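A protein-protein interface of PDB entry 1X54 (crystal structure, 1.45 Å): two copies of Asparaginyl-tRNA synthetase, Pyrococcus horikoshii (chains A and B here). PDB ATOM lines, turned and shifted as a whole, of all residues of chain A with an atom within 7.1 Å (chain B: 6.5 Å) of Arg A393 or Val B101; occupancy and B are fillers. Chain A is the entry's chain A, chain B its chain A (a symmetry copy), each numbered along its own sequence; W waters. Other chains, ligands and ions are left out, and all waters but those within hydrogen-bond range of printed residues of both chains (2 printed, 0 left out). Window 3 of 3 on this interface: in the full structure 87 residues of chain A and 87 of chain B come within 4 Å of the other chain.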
ATOM      1  N   ASP A 366       1.084   8.350 -11.513  1.00  0.00           N
ATOM      2  CA  ASP A 366      -0.075   7.497 -11.770  1.00  0.00           C
ATOM      3  C   ASP A 366      -1.401   8.130 -11.349  1.00  0.00           C
ATOM      4  O   ASP A 366      -2.469   7.520 -11.498  1.00  0.00           O
ATOM      5  CB  ASP A 366       0.105   6.122 -11.118  1.00  0.00           C
ATOM      6  CG  ASP A 366       0.480   6.210  -9.657  1.00  0.00           C
ATOM      7  OD1 ASP A 366      -0.004   7.137  -8.955  1.00  0.00           O
ATOM      8  OD2 ASP A 366       1.233   5.384  -9.108  1.00  0.00           O
ATOM      9  N   TYR A 368      -4.120  11.003 -12.059  1.00  0.00           N
ATOM     10  CA  TYR A 368      -4.583  11.869 -13.135  1.00  0.00           C
ATOM     11  C   TYR A 368      -4.426  13.367 -12.826  1.00  0.00           C
ATOM     12  O   TYR A 368      -3.862  14.119 -13.632  1.00  0.00           O
ATOM     13  CB  TYR A 368      -6.048  11.556 -13.480  1.00  0.00           C
ATOM     14  CG  TYR A 368      -6.624  12.451 -14.547  1.00  0.00           C
ATOM     15  CD1 TYR A 368      -7.210  13.680 -14.214  1.00  0.00           C
ATOM     16  CD2 TYR A 368      -6.595  12.082 -15.887  1.00  0.00           C
ATOM     17  CE1 TYR A 368      -7.734  14.506 -15.189  1.00  0.00           C
ATOM     18  CE2 TYR A 368      -7.122  12.904 -16.871  1.00  0.00           C
ATOM     19  CZ  TYR A 368      -7.692  14.112 -16.516  1.00  0.00           C
ATOM     20  OH  TYR A 368      -8.216  14.928 -17.499  1.00  0.00           O
ATOM     21  N   GLU A 386      -3.689  13.862 -24.292  1.00  0.00           N
ATOM     22  CA  GLU A 386      -4.951  13.341 -23.783  1.00  0.00           C
ATOM     23  C   GLU A 386      -4.898  11.815 -23.659  1.00  0.00           C
ATOM     24  O   GLU A 386      -5.382  11.251 -22.678  1.00  0.00           O
ATOM     25  CB  GLU A 386      -6.124  13.755 -24.683  1.00  0.00           C
ATOM     26  CG  GLU A 386      -7.484  13.386 -24.104  1.00  0.00           C
ATOM     27  CD  GLU A 386      -8.655  13.620 -25.054  1.00  0.00           C
ATOM     28  OE1 GLU A 386      -8.500  14.359 -26.062  1.00  0.00           O
ATOM     29  OE2 GLU A 386      -9.738  13.044 -24.790  1.00  0.00           O
ATOM     30  N   TYR A 388      -2.343   9.966 -23.156  1.00  0.00           N
ATOM     31  CA  TYR A 388      -1.427   9.621 -22.077  1.00  0.00           C
ATOM     32  C   TYR A 388      -2.114   9.818 -20.719  1.00  0.00           C
ATOM     33  O   TYR A 388      -1.980   8.993 -19.805  1.00  0.00           O
ATOM     34  CB  TYR A 388      -0.169  10.484 -22.213  1.00  0.00           C
ATOM     35  CG  TYR A 388       0.945  10.145 -21.261  1.00  0.00           C
ATOM     36  CD1 TYR A 388       1.575   8.906 -21.305  1.00  0.00           C
ATOM     37  CD2 TYR A 388       1.393  11.089 -20.326  1.00  0.00           C
ATOM     38  CE1 TYR A 388       2.606   8.609 -20.429  1.00  0.00           C
ATOM     39  CE2 TYR A 388       2.409  10.794 -19.454  1.00  0.00           C
ATOM     40  CZ  TYR A 388       3.018   9.555 -19.506  1.00  0.00           C
ATOM     41  OH  TYR A 388       4.053   9.284 -18.639  1.00  0.00           O
ATOM     42  N   LEU A 389      -2.886  10.895 -20.610  1.00  0.00           N
ATOM     43  CA  LEU A 389      -3.744  11.129 -19.451  1.00  0.00           C
ATOM     44  C   LEU A 389      -4.800  10.031 -19.292  1.00  0.00           C
ATOM     45  O   LEU A 389      -5.155   9.658 -18.169  1.00  0.00           O
ATOM     46  CB  LEU A 389      -4.406  12.522 -19.542  1.00  0.00           C
ATOM     47  CG  LEU A 389      -3.454  13.680 -19.225  1.00  0.00           C
ATOM     48  CD1 LEU A 389      -3.918  15.009 -19.878  1.00  0.00           C
ATOM     49  CD2 LEU A 389      -3.298  13.835 -17.724  1.00  0.00           C
ATOM     50  N   ASP A 390      -5.304   9.513 -20.414  1.00  0.00           N
ATOM     51  CA  ASP A 390      -6.269   8.390 -20.393  1.00  0.00           C
ATOM     52  C   ASP A 390      -5.752   7.182 -19.603  1.00  0.00           C
ATOM     53  O   ASP A 390      -6.539   6.434 -18.999  1.00  0.00           O
ATOM     54  CB  ASP A 390      -6.591   7.904 -21.807  1.00  0.00           C
ATOM     55  CG  ASP A 390      -7.653   8.743 -22.521  1.00  0.00           C
ATOM     56  OD1 ASP A 390      -8.358   9.577 -21.876  1.00  0.00           O
ATOM     57  OD2 ASP A 390      -7.837   8.600 -23.752  1.00  0.00           O
ATOM     58  N   LEU A 391      -4.438   6.967 -19.652  1.00  0.00           N
ATOM     59  CA  LEU A 391      -3.839   5.865 -18.897  1.00  0.00           C
ATOM     60  C   LEU A 391      -3.976   6.014 -17.381  1.00  0.00           C
ATOM     61  O   LEU A 391      -3.767   5.053 -16.627  1.00  0.00           O
ATOM     62  CB  LEU A 391      -2.380   5.634 -19.317  1.00  0.00           C
ATOM     63  CG  LEU A 391      -2.127   5.536 -20.822  1.00  0.00           C
ATOM     64  CD1 LEU A 391      -0.619   5.467 -21.018  1.00  0.00           C
ATOM     65  CD2 LEU A 391      -2.821   4.284 -21.389  1.00  0.00           C
ATOM     66  N   ARG A 392      -4.295   7.229 -16.935  1.00  0.00           N
ATOM     67  CA  ARG A 392      -4.568   7.487 -15.526  1.00  0.00           C
ATOM     68  C   ARG A 392      -6.080   7.531 -15.225  1.00  0.00           C
ATOM     69  O   ARG A 392      -6.486   7.815 -14.080  1.00  0.00           O
ATOM     70  CB  ARG A 392      -3.906   8.799 -15.073  1.00  0.00           C
ATOM     71  CG  ARG A 392      -2.399   8.756 -14.873  1.00  0.00           C
ATOM     72  CD  ARG A 392      -1.616   8.581 -16.165  1.00  0.00           C
ATOM     73  NE  ARG A 392      -0.186   8.511 -15.899  1.00  0.00           N
ATOM     74  CZ  ARG A 392       0.730   8.268 -16.824  1.00  0.00           C
ATOM     75  NH1 ARG A 392       0.368   8.105 -18.099  1.00  0.00           N
ATOM     76  NH2 ARG A 392       2.015   8.200 -16.463  1.00  0.00           N
ATOM     77  N   ARG A 393      -6.893   7.251 -16.240  1.00  0.00           N
ATOM     78  CA  ARG A 393      -8.356   7.290 -16.109  1.00  0.00           C
ATOM     79  C   ARG A 393      -8.980   5.879 -16.180  1.00  0.00           C
ATOM     80  O   ARG A 393     -10.030   5.617 -15.590  1.00  0.00           O
ATOM     81  CB  ARG A 393      -8.912   8.194 -17.211  1.00  0.00           C
ATOM     82  CG  ARG A 393     -10.405   8.349 -17.296  1.00  0.00           C
ATOM     83  CD  ARG A 393     -10.831   9.290 -18.431  1.00  0.00           C
ATOM     84  NE  ARG A 393     -10.410  10.676 -18.237  1.00  0.00           N
ATOM     85  CZ  ARG A 393     -11.167  11.597 -17.627  1.00  0.00           C
ATOM     86  NH1 ARG A 393     -10.739  12.850 -17.493  1.00  0.00           N
ATOM     87  NH2 ARG A 393     -12.359  11.258 -17.139  1.00  0.00           N
ATOM     88  N   TYR A 394      -8.336   4.981 -16.919  1.00  0.00           N
ATOM     89  CA  TYR A 394      -8.956   3.687 -17.222  1.00  0.00           C
ATOM     90  C   TYR A 394      -8.216   2.505 -16.604  1.00  0.00           C
ATOM     91  O   TYR A 394      -7.861   1.553 -17.305  1.00  0.00           O
ATOM     92  CB  TYR A 394      -9.148   3.512 -18.732  1.00  0.00           C
ATOM     93  CG  TYR A 394     -10.014   4.592 -19.337  1.00  0.00           C
ATOM     94  CD1 TYR A 394     -11.359   4.712 -18.968  1.00  0.00           C
ATOM     95  CD2 TYR A 394      -9.497   5.504 -20.265  1.00  0.00           C
ATOM     96  CE1 TYR A 394     -12.167   5.692 -19.507  1.00  0.00           C
ATOM     97  CE2 TYR A 394     -10.303   6.490 -20.809  1.00  0.00           C
ATOM     98  CZ  TYR A 394     -11.634   6.579 -20.422  1.00  0.00           C
ATOM     99  OH  TYR A 394     -12.441   7.548 -20.961  1.00  0.00           O
ATOM    100  N   GLY A 395      -8.014   2.555 -15.290  1.00  0.00           N
ATOM    101  CA  GLY A 395      -7.407   1.456 -14.563  1.00  0.00           C
ATOM    102  C   GLY A 395      -5.938   1.720 -14.302  1.00  0.00           C
ATOM    103  O   GLY A 395      -5.077   0.841 -14.509  1.00  0.00           O
ATOM    104  N   SER A 396      -5.646   2.952 -13.884  1.00  0.00           N
ATOM    105  CA  SER A 396      -4.286   3.335 -13.521  1.00  0.00           C
ATOM    106  C   SER A 396      -3.634   2.329 -12.573  1.00  0.00           C
ATOM    107  O   SER A 396      -4.289   1.781 -11.664  1.00  0.00           O
ATOM    108  CB  SER A 396      -4.298   4.715 -12.861  1.00  0.00           C
ATOM    109  OG  SER A 396      -2.976   5.207 -12.795  1.00  0.00           O
ATOM    110  N   LYS B  65     -19.435  -2.222  -7.843  1.00  0.00           N
ATOM    111  CA  LYS B  65     -19.296  -1.044  -8.694  1.00  0.00           C
ATOM    112  C   LYS B  65     -18.138  -1.126  -9.697  1.00  0.00           C
ATOM    113  O   LYS B  65     -17.888  -0.176 -10.443  1.00  0.00           O
ATOM    114  CB  LYS B  65     -19.161   0.206  -7.819  1.00  0.00           C
ATOM    115  CG  LYS B  65     -20.380   0.461  -6.928  1.00  0.00           C
ATOM    116  CD  LYS B  65     -20.548   1.939  -6.525  1.00  0.00           C
ATOM    117  CE  LYS B  65     -19.267   2.563  -5.941  1.00  0.00           C
ATOM    118  NZ  LYS B  65     -18.786   1.901  -4.692  1.00  0.00           N
ATOM    119  N   LEU B  66     -17.420  -2.244  -9.707  1.00  0.00           N
ATOM    120  CA  LEU B  66     -16.252  -2.361 -10.576  1.00  0.00           C
ATOM    121  C   LEU B  66     -16.634  -2.746 -11.989  1.00  0.00           C
ATOM    122  O   LEU B  66     -17.067  -3.882 -12.239  1.00  0.00           O
ATOM    123  CB  LEU B  66     -15.244  -3.360 -10.018  1.00  0.00           C
ATOM    124  CG  LEU B  66     -14.744  -3.021  -8.619  1.00  0.00           C
ATOM    125  CD1 LEU B  66     -13.817  -4.125  -8.140  1.00  0.00           C
ATOM    126  CD2 LEU B  66     -14.066  -1.651  -8.574  1.00  0.00           C
ATOM    127  N   GLY B  67     -16.452  -1.802 -12.906  1.00  0.00           N
ATOM    128  CA  GLY B  67     -16.684  -2.057 -14.307  1.00  0.00           C
ATOM    129  C   GLY B  67     -15.403  -2.521 -14.984  1.00  0.00           C
ATOM    130  O   GLY B  67     -14.334  -2.652 -14.344  1.00  0.00           O
ATOM    131  N   ARG B  68     -15.516  -2.767 -16.282  1.00  0.00           N
ATOM    132  CA  ARG B  68     -14.398  -3.235 -17.089  1.00  0.00           C
ATOM    133  C   ARG B  68     -13.234  -2.265 -17.006  1.00  0.00           C
ATOM    134  O   ARG B  68     -13.404  -1.037 -17.084  1.00  0.00           O
ATOM    135  CB  ARG B  68     -14.813  -3.387 -18.550  1.00  0.00           C
ATOM    136  CG  ARG B  68     -15.852  -4.475 -18.794  1.00  0.00           C
ATOM    137  CD  ARG B  68     -16.305  -4.607 -20.251  1.00  0.00           C
ATOM    138  NE  ARG B  68     -16.536  -3.318 -20.899  1.00  0.00           N
ATOM    139  CZ  ARG B  68     -15.829  -2.877 -21.938  1.00  0.00           C
ATOM    140  NH1 ARG B  68     -14.847  -3.620 -22.442  1.00  0.00           N
ATOM    141  NH2 ARG B  68     -16.098  -1.695 -22.461  1.00  0.00           N
ATOM    142  N   GLU B  69     -12.056  -2.863 -16.850  1.00  0.00           N
ATOM    143  CA  GLU B  69     -10.765  -2.181 -16.754  1.00  0.00           C
ATOM    144  C   GLU B  69     -10.477  -1.524 -15.408  1.00  0.00           C
ATOM    145  O   GLU B  69      -9.448  -0.863 -15.255  1.00  0.00           O
ATOM    146  CB  GLU B  69     -10.497  -1.237 -17.951  1.00  0.00           C
ATOM    147  CG  GLU B  69     -10.390  -1.997 -19.274  1.00  0.00           C
ATOM    148  CD  GLU B  69      -9.274  -3.032 -19.279  1.00  0.00           C
ATOM    149  OE1 GLU B  69      -8.148  -2.693 -18.866  1.00  0.00           O
ATOM    150  OE2 GLU B  69      -9.506  -4.166 -19.737  1.00  0.00           O
ATOM    151  N   SER B  70     -11.359  -1.732 -14.422  1.00  0.00           N
ATOM    152  CA  SER B  70     -11.000  -1.362 -13.061  1.00  0.00           C
ATOM    153  C   SER B  70      -9.713  -2.080 -12.657  1.00  0.00           C
ATOM    154  O   SER B  70      -9.591  -3.289 -12.837  1.00  0.00           O
ATOM    155  CB  SER B  70     -12.085  -1.755 -12.063  1.00  0.00           C
ATOM    156  OG  SER B  70     -13.319  -1.110 -12.325  1.00  0.00           O
ATOM    157  N   SER B  71      -8.759  -1.339 -12.111  1.00  0.00           N
ATOM    158  CA  SER B  71      -7.504  -1.957 -11.671  1.00  0.00           C
ATOM    159  C   SER B  71      -7.624  -2.406 -10.229  1.00  0.00           C
ATOM    160  O   SER B  71      -8.084  -1.643  -9.364  1.00  0.00           O
ATOM    161  CB  SER B  71      -6.325  -1.001 -11.887  1.00  0.00           C
ATOM    162  OG  SER B  71      -6.584   0.264 -11.313  1.00  0.00           O
ATOM    163  N   VAL B  97      -9.063  -1.980  -4.423  1.00  0.00           N
ATOM    164  CA  VAL B  97      -9.411  -1.293  -5.647  1.00  0.00           C
ATOM    165  C   VAL B  97      -8.402  -0.184  -5.863  1.00  0.00           C
ATOM    166  O   VAL B  97      -8.301   0.768  -5.049  1.00  0.00           O
ATOM    167  CB  VAL B  97     -10.831  -0.697  -5.595  1.00  0.00           C
ATOM    168  CG1 VAL B  97     -11.128   0.053  -6.891  1.00  0.00           C
ATOM    169  CG2 VAL B  97     -11.856  -1.815  -5.345  1.00  0.00           C
ATOM    170  N   GLN B  99      -8.093   1.604  -9.036  1.00  0.00           N
ATOM    171  CA  GLN B  99      -8.975   2.572  -9.660  1.00  0.00           C
ATOM    172  C   GLN B  99     -10.204   1.884 -10.245  1.00  0.00           C
ATOM    173  O   GLN B  99     -10.080   1.034 -11.132  1.00  0.00           O
ATOM    174  CB  GLN B  99      -8.244   3.342 -10.753  1.00  0.00           C
ATOM    175  CG  GLN B  99      -9.109   4.398 -11.405  1.00  0.00           C
ATOM    176  CD  GLN B  99      -8.366   5.200 -12.446  1.00  0.00           C
ATOM    177  OE1 GLN B  99      -7.786   4.633 -13.383  1.00  0.00           O
ATOM    178  NE2 GLN B  99      -8.372   6.526 -12.291  1.00  0.00           N
ATOM    179  N   ALA B 100     -11.381   2.247  -9.744  1.00  0.00           N
ATOM    180  CA  ALA B 100     -12.641   1.808 -10.337  1.00  0.00           C
ATOM    181  C   ALA B 100     -12.900   2.523 -11.667  1.00  0.00           C
ATOM    182  O   ALA B 100     -12.633   3.731 -11.818  1.00  0.00           O
ATOM    183  CB  ALA B 100     -13.793   2.057  -9.377  1.00  0.00           C
ATOM    184  N   VAL B 101     -13.405   1.758 -12.631  1.00  0.00           N
ATOM    185  CA  VAL B 101     -13.723   2.253 -13.957  1.00  0.00           C
ATOM    186  C   VAL B 101     -15.122   1.777 -14.318  1.00  0.00           C
ATOM    187  O   VAL B 101     -15.469   0.629 -14.055  1.00  0.00           O
ATOM    188  CB  VAL B 101     -12.711   1.716 -14.995  1.00  0.00           C
ATOM    189  CG1 VAL B 101     -13.056   2.179 -16.412  1.00  0.00           C
ATOM    190  CG2 VAL B 101     -11.285   2.127 -14.622  1.00  0.00           C
ATOM    191  N   SER B 102     -15.908   2.652 -14.933  1.00  0.00           N
ATOM    192  CA  SER B 102     -17.234   2.254 -15.405  1.00  0.00           C
ATOM    193  C   SER B 102     -17.500   2.558 -16.882  1.00  0.00           C
ATOM    194  O   SER B 102     -18.451   2.022 -17.462  1.00  0.00           O
ATOM    195  CB  SER B 102     -18.318   2.879 -14.525  1.00  0.00           C
ATOM    196  OG  SER B 102     -18.247   4.290 -14.560  1.00  0.00           O
ATOM    197  N   GLU B 103     -16.670   3.397 -17.496  1.00  0.00           N
ATOM    198  CA  GLU B 103     -16.931   3.840 -18.871  1.00  0.00           C
ATOM    199  C   GLU B 103     -15.760   3.617 -19.836  1.00  0.00           C
ATOM    200  O   GLU B 103     -15.400   4.503 -20.616  1.00  0.00           O
ATOM    201  CB  GLU B 103     -17.348   5.316 -18.900  1.00  0.00           C
ATOM    202  CG  GLU B 103     -18.487   5.691 -17.960  1.00  0.00           C
ATOM    203  CD  GLU B 103     -18.793   7.177 -18.003  1.00  0.00           C
ATOM    204  OE1 GLU B 103     -19.414   7.623 -18.999  1.00  0.00           O
ATOM    205  OE2 GLU B 103     -18.409   7.898 -17.049  1.00  0.00           O
ATOM    206  N   PHE B 104     -15.172   2.428 -19.806  1.00  0.00           N
ATOM    207  CA  PHE B 104     -14.103   2.130 -20.755  1.00  0.00           C
ATOM    208  C   PHE B 104     -14.640   2.264 -22.185  1.00  0.00           C
ATOM    209  O   PHE B 104     -15.648   1.630 -22.508  1.00  0.00           O
ATOM    210  CB  PHE B 104     -13.566   0.726 -20.506  1.00  0.00           C
ATOM    211  CG  PHE B 104     -12.288   0.429 -21.237  1.00  0.00           C
ATOM    212  CD1 PHE B 104     -11.141   1.184 -20.996  1.00  0.00           C
ATOM    213  CD2 PHE B 104     -12.221  -0.620 -22.147  1.00  0.00           C
ATOM    214  CE1 PHE B 104      -9.961   0.900 -21.662  1.00  0.00           C
ATOM    215  CE2 PHE B 104     -11.046  -0.899 -22.815  1.00  0.00           C
ATOM    216  CZ  PHE B 104      -9.912  -0.128 -22.568  1.00  0.00           C
HETATM  217  O   HOH W   1     -15.196   7.069 -21.152  1.00  0.00           O
HETATM  218  O   HOH W   2      -5.774   8.659 -11.541  1.00  0.00           O
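No position is printed for both chains.
O of Arg A392 is in hydrogen-bond range of NE2 of Gln B99. O of Arg A393 lies close to OE1 of Gln B99 (3.3 Å). OE1 of Gln B99 lies within hydrogen-bond range of N of Gly A395 (2.8 Å). The backbone carbonyl oxygen (O) of Ser A396 lies within hydrogen-bond range of the side-chain hydroxyl (OG) of Ser B71. The backbone NH of Ser A396 sits at hydrogen-bond distance from the side-chain amide oxygen of Gln B99 (2.8 Å).
Arg A393 touches two residues of chain B. Of chain A, only Arg A393, Tyr A394 and Gly A395 come within 4 Å of Val B101. Printed residues of chain B within 4 Å of Tyr A394: Glu B69, Gln B99, Val B101, Glu B103 and Phe B104. Of the printed residues of chain A, Glu B103 touches Tyr A394. Val B97 touches none of the printed residues of chain A. Ser B102 touches none of the printed residues of chain A. The nearest residue of chain A that does not touch Val B101 is Ser A396 (5.7 Å).
Water W1 bridges the backbone carbonyl oxygen of Glu B103 (2.6 Å) and the side-chain hydroxyl of Tyr A394 (2.8 Å). Water W2 lies within hydrogen-bond range of the backbone carbonyl oxygen (O) of Arg A392 (2.8 Å), the backbone NH (N) of Tyr A368 (2.9 Å), the side-chain amide nitrogen (NE2) of Gln B99 (3.4 Å) and the backbone carbonyl oxygen (O) of Asp A366 (3.5 Å).
Arg A393 touches Val B101 (O to CG2, 3.8 Å). O of Tyr A394 touches O of Glu B69, 3.5 Å away. Gln B99 touches Tyr A394. CG2 of Val B101 touches C of Tyr A394 (3.7 Å). Glu B103 touches Tyr A394. Phe B104 touches Tyr A394. Gly A395 touches Glu B69. Gly A395 touches Ser B71 (C to OG, 3.4 Å). Gly A395 touches Val B101.
Of the 12 printed residues of chain A, 5 touch a printed residue of chain B. Among the printed residues, no Asp or Glu carboxylate lies within 4 Å of a Lys or Arg side-chain nitrogen of the other chain.
The side-chain hydroxyl (OG) of Ser A396 sits at hydrogen-bond distance from the backbone carbonyl oxygen (O) of Asp A366, at 2.7 Å. NH1 of Arg A392 is in hydrogen-bond range of O of Tyr A388 (3.0 Å). N of Gly B67 lies within hydrogen-bond range of O of Val B101, 2.9 Å away. NH2 of Arg B68 is in hydrogen-bond range of O of Phe B104 (3.4 Å). OG of Ser B70 lies within hydrogen-bond range of N of Val B101 (2.9 Å). O of Gln B99 lies within hydrogen-bond range of N of Ser B71, 2.9 Å away.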
